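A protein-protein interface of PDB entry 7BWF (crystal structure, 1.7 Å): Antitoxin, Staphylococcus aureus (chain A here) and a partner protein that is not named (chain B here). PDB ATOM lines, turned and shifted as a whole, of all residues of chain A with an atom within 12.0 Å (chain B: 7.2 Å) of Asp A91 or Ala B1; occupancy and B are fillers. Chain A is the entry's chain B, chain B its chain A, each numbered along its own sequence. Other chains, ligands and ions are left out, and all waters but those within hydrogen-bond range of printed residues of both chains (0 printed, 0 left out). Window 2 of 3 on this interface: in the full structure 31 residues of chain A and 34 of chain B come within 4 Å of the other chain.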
ATOM      1  N   THR A  87       9.038  29.629 -20.963  1.00  0.00           N
ATOM      2  CA  THR A  87       9.116  29.609 -19.510  1.00  0.00           C
ATOM      3  C   THR A  87       8.236  30.710 -18.936  1.00  0.00           C
ATOM      4  O   THR A  87       8.370  31.884 -19.306  1.00  0.00           O
ATOM      5  CB  THR A  87      10.555  29.794 -19.031  1.00  0.00           C
ATOM      6  OG1 THR A  87      11.426  28.954 -19.798  1.00  0.00           O
ATOM      7  CG2 THR A  87      10.680  29.416 -17.559  1.00  0.00           C
ATOM      8  N   LYS A  88       7.346  30.322 -18.029  1.00  0.00           N
ATOM      9  CA  LYS A  88       6.338  31.210 -17.481  1.00  0.00           C
ATOM     10  C   LYS A  88       6.181  30.909 -15.999  1.00  0.00           C
ATOM     11  O   LYS A  88       6.164  29.746 -15.590  1.00  0.00           O
ATOM     12  CB  LYS A  88       4.996  31.023 -18.202  1.00  0.00           C
ATOM     13  CG  LYS A  88       4.938  31.578 -19.624  1.00  0.00           C
ATOM     14  CD  LYS A  88       5.390  33.038 -19.738  1.00  0.00           C
ATOM     15  CE  LYS A  88       4.458  33.820 -20.663  1.00  0.00           C
ATOM     16  NZ  LYS A  88       5.132  34.279 -21.910  1.00  0.00           N
ATOM     17  N   ASP A  89       6.081  31.963 -15.203  1.00  0.00           N
ATOM     18  CA  ASP A  89       5.582  31.836 -13.844  1.00  0.00           C
ATOM     19  C   ASP A  89       4.077  31.606 -13.886  1.00  0.00           C
ATOM     20  O   ASP A  89       3.335  32.438 -14.417  1.00  0.00           O
ATOM     21  CB  ASP A  89       5.894  33.103 -13.056  1.00  0.00           C
ATOM     22  CG  ASP A  89       7.306  33.118 -12.505  1.00  0.00           C
ATOM     23  OD1 ASP A  89       8.051  32.132 -12.675  1.00  0.00           O
ATOM     24  OD2 ASP A  89       7.679  34.154 -11.931  1.00  0.00           O
ATOM     25  N   ILE A  90       3.630  30.476 -13.340  1.00  0.00           N
ATOM     26  CA  ILE A  90       2.208  30.199 -13.157  1.00  0.00           C
ATOM     27  C   ILE A  90       1.919  30.084 -11.666  1.00  0.00           C
ATOM     28  O   ILE A  90       2.706  29.493 -10.914  1.00  0.00           O
ATOM     29  CB  ILE A  90       1.762  28.919 -13.896  1.00  0.00           C
ATOM     30  CG1 ILE A  90       2.176  27.657 -13.135  1.00  0.00           C
ATOM     31  CG2 ILE A  90       2.351  28.917 -15.300  1.00  0.00           C
ATOM     32  CD1 ILE A  90       1.849  26.357 -13.872  1.00  0.00           C
ATOM     33  N   ASP A  91       0.785  30.650 -11.242  1.00  0.00           N
ATOM     34  CA  ASP A  91       0.377  30.573  -9.846  1.00  0.00           C
ATOM     35  C   ASP A  91      -0.349  29.261  -9.604  1.00  0.00           C
ATOM     36  O   ASP A  91      -1.324  28.947 -10.288  1.00  0.00           O
ATOM     37  CB  ASP A  91      -0.523  31.741  -9.450  1.00  0.00           C
ATOM     38  CG  ASP A  91      -0.624  31.889  -7.932  1.00  0.00           C
ATOM     39  OD1 ASP A  91       0.398  31.657  -7.252  1.00  0.00           O
ATOM     40  OD2 ASP A  91      -1.704  32.224  -7.418  1.00  0.00           O
ATOM     41  N   VAL A  92       0.136  28.502  -8.633  1.00  0.00           N
ATOM     42  CA  VAL A  92      -0.328  27.152  -8.401  1.00  0.00           C
ATOM     43  C   VAL A  92      -0.799  27.024  -6.951  1.00  0.00           C
ATOM     44  O   VAL A  92      -1.030  28.022  -6.262  1.00  0.00           O
ATOM     45  CB  VAL A  92       0.789  26.146  -8.717  1.00  0.00           C
ATOM     46  CG1 VAL A  92       0.606  24.909  -7.909  1.00  0.00           C
ATOM     47  CG2 VAL A  92       0.843  25.809 -10.213  1.00  0.00           C
ATOM     48  N   ALA B   1       1.068  30.616  -4.933  1.00  0.00           N
ATOM     49  CA  ALA B   1       2.405  30.029  -4.949  1.00  0.00           C
ATOM     50  C   ALA B   1       3.031  30.024  -6.343  1.00  0.00           C
ATOM     51  O   ALA B   1       2.767  29.141  -7.170  1.00  0.00           O
ATOM     52  CB  ALA B   1       2.354  28.612  -4.393  1.00  0.00           C
ATOM     53  N   ARG B   2       3.879  31.020  -6.587  1.00  0.00           N
ATOM     54  CA  ARG B   2       4.573  31.121  -7.859  1.00  0.00           C
ATOM     55  C   ARG B   2       5.379  29.857  -8.105  1.00  0.00           C
ATOM     56  O   ARG B   2       6.104  29.385  -7.223  1.00  0.00           O
ATOM     57  CB  ARG B   2       5.484  32.349  -7.857  1.00  0.00           C
ATOM     58  CG  ARG B   2       6.158  32.675  -9.183  1.00  0.00           C
ATOM     59  CD  ARG B   2       7.299  33.679  -8.971  1.00  0.00           C
ATOM     60  NE  ARG B   2       8.320  33.139  -8.077  1.00  0.00           N
ATOM     61  CZ  ARG B   2       9.448  32.563  -8.483  1.00  0.00           C
ATOM     62  NH1 ARG B   2       9.717  32.461  -9.780  1.00  0.00           N
ATOM     63  NH2 ARG B   2      10.313  32.091  -7.596  1.00  0.00           N
ATOM     64  N   LEU B   3       5.215  29.299  -9.300  1.00  0.00           N
ATOM     65  CA  LEU B   3       5.955  28.124  -9.741  1.00  0.00           C
ATOM     66  C   LEU B   3       6.458  28.388 -11.150  1.00  0.00           C
ATOM     67  O   LEU B   3       5.655  28.615 -12.062  1.00  0.00           O
ATOM     68  CB  LEU B   3       5.072  26.874  -9.719  1.00  0.00           C
ATOM     69  CG  LEU B   3       5.735  25.493  -9.754  1.00  0.00           C
ATOM     70  CD1 LEU B   3       6.884  25.368  -8.755  1.00  0.00           C
ATOM     71  CD2 LEU B   3       4.681  24.398  -9.508  1.00  0.00           C
ATOM     72  N   ASN B   4       7.778  28.366 -11.326  1.00  0.00           N
ATOM     73  CA  ASN B   4       8.387  28.570 -12.634  1.00  0.00           C
ATOM     74  C   ASN B   4       8.372  27.250 -13.392  1.00  0.00           C
ATOM     75  O   ASN B   4       8.952  26.257 -12.936  1.00  0.00           O
ATOM     76  CB  ASN B   4       9.814  29.097 -12.514  1.00  0.00           C
ATOM     77  CG  ASN B   4      10.299  29.731 -13.803  1.00  0.00           C
ATOM     78  OD1 ASN B   4      11.152  29.183 -14.504  1.00  0.00           O
ATOM     79  ND2 ASN B   4       9.734  30.886 -14.136  1.00  0.00           N
ATOM     80  N   TYR B  15      -2.031  24.373 -22.776  1.00  0.00           N
ATOM     81  CA  TYR B  15      -2.246  24.996 -21.474  1.00  0.00           C
ATOM     82  C   TYR B  15      -3.057  26.279 -21.622  1.00  0.00           C
ATOM     83  O   TYR B  15      -4.069  26.474 -20.939  1.00  0.00           O
ATOM     84  CB  TYR B  15      -0.900  25.275 -20.800  1.00  0.00           C
ATOM     85  CG  TYR B  15      -1.039  25.662 -19.348  1.00  0.00           C
ATOM     86  CD1 TYR B  15      -1.237  24.699 -18.369  1.00  0.00           C
ATOM     87  CD2 TYR B  15      -0.987  26.990 -18.959  1.00  0.00           C
ATOM     88  CE1 TYR B  15      -1.368  25.049 -17.041  1.00  0.00           C
ATOM     89  CE2 TYR B  15      -1.116  27.350 -17.635  1.00  0.00           C
ATOM     90  CZ  TYR B  15      -1.306  26.376 -16.676  1.00  0.00           C
ATOM     91  OH  TYR B  15      -1.437  26.721 -15.348  1.00  0.00           O
ATOM     92  N   ASN B  30      -2.526  22.233 -12.668  1.00  0.00           N
ATOM     93  CA  ASN B  30      -1.794  22.997 -11.663  1.00  0.00           C
ATOM     94  C   ASN B  30      -1.612  22.181 -10.391  1.00  0.00           C
ATOM     95  O   ASN B  30      -0.574  22.281  -9.724  1.00  0.00           O
ATOM     96  CB  ASN B  30      -2.523  24.306 -11.359  1.00  0.00           C
ATOM     97  CG  ASN B  30      -2.383  25.324 -12.471  1.00  0.00           C
ATOM     98  OD1 ASN B  30      -1.647  25.118 -13.436  1.00  0.00           O
ATOM     99  ND2 ASN B  30      -3.110  26.427 -12.350  1.00  0.00           N
ATOM    100  N   LYS B  34       1.990  21.176  -8.694  1.00  0.00           N
ATOM    101  CA  LYS B  34       2.274  21.354  -7.273  1.00  0.00           C
ATOM    102  C   LYS B  34       2.759  20.050  -6.644  1.00  0.00           C
ATOM    103  O   LYS B  34       3.750  20.028  -5.908  1.00  0.00           O
ATOM    104  CB  LYS B  34       1.022  21.870  -6.557  1.00  0.00           C
ATOM    105  CG  LYS B  34       1.328  22.696  -5.326  1.00  0.00           C
ATOM    106  CD  LYS B  34       0.190  23.663  -5.041  1.00  0.00           C
ATOM    107  CE  LYS B  34      -0.710  23.158  -3.928  1.00  0.00           C
ATOM    108  NZ  LYS B  34      -2.057  23.795  -3.967  1.00  0.00           N
ATOM    109  N   ARG B  38       6.448  19.412  -4.798  1.00  0.00           N
ATOM    110  CA  ARG B  38       6.621  19.067  -3.393  1.00  0.00           C
ATOM    111  C   ARG B  38       7.152  17.648  -3.239  1.00  0.00           C
ATOM    112  O   ARG B  38       8.037  17.392  -2.416  1.00  0.00           O
ATOM    113  CB  ARG B  38       5.288  19.213  -2.651  1.00  0.00           C
ATOM    114  CG  ARG B  38       4.661  20.582  -2.720  1.00  0.00           C
ATOM    115  CD  ARG B  38       3.586  20.679  -1.659  1.00  0.00           C
ATOM    116  NE  ARG B  38       3.066  22.026  -1.498  1.00  0.00           N
ATOM    117  CZ  ARG B  38       1.833  22.313  -1.091  1.00  0.00           C
ATOM    118  NH1 ARG B  38       1.462  23.582  -0.979  1.00  0.00           N
ATOM    119  NH2 ARG B  38       0.966  21.347  -0.797  1.00  0.00           N
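The side-chain carboxylate (OD1) of Asp A89 sits at hydrogen-bond distance from the side-chain amide nitrogen (ND2) of Asn B4.
The backbone carbonyl oxygen (O) of Ile A90 lies within hydrogen-bond range of the backbone NH (N) of Leu B3, 3.0 Å away.
The guanidinium group of Arg B2 is in salt-bridge range of the side-chain carboxylate of Asp A89 (3.4 Å).
OD1 of Asp A91 is in hydrogen-bond range of N of Ala B1, at 2.6 Å.
The backbone NH (N) of Val A92 sits at hydrogen-bond distance from the backbone carbonyl oxygen (O) of Ala B1, at 3.1 Å.
The side-chain hydroxyl (OH) of Tyr B15 lies within hydrogen-bond range of the side-chain amide oxygen (OD1) of Asn B30.
O of Lys A88 touches O of Leu B3, 3.7 Å away.
Lys A88 touches Asn B4.
Leu B3 touches Asp A89.
Ile A90 touches Ala B1.
O of Ile A90 touches C of Arg B2 (3.9 Å).
Ile A90 touches Tyr B15 (CD1 to OH, 3.6 Å).
OD1 of Asn B30 touches CD1 of Ile A90, 3.7 Å away.
OD1 of Asp A91 touches N of Arg B2, 3.6 Å away.
Asn B30 touches Asp A91.
Val A92 touches Lys B34.
Printed residues of chain B within 4 Å of Asp A91: Ala B1, Arg B2 and Asn B30.
Ala B1 touches three residues of chain A.
Arg B2 touches three residues of chain A.
Leu B3 touches three residues of chain A.
Of chain A, only Ile A90 (3.7 Å), Asp A91 (3.7 Å) and Val A92 (3.4 Å) come within 4 Å of Asn B30.
Of the printed residues of chain B, Thr A87 touches Asn B4.
Printed residues of chain A within 4 Å of Asn B4: Thr A87, Lys A88 and Asp A89.
Of the printed residues of chain B, Lys A88 touches Leu B3 (3.7 Å) and Asn B4 (3.9 Å).
The nearest printed residue of chain A that does not touch Lys B34 is Asp A91 (7.2 Å).
Of the 6 printed residues of chain A, 6 touch a printed residue of chain B.
Hydrophobic or aromatic side chains of chain A within 4 Å of the printed part of chain B: Ile A90 and Val A92.
Along chain A the printed residues that touch a printed residue of chain B span positions 87 to 92.
Among the printed residues, Asp or Glu carboxylates within 4 Å of a Lys or Arg side-chain nitrogen of the other chain: Asp A89 with Arg B2 (3.4 Å).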
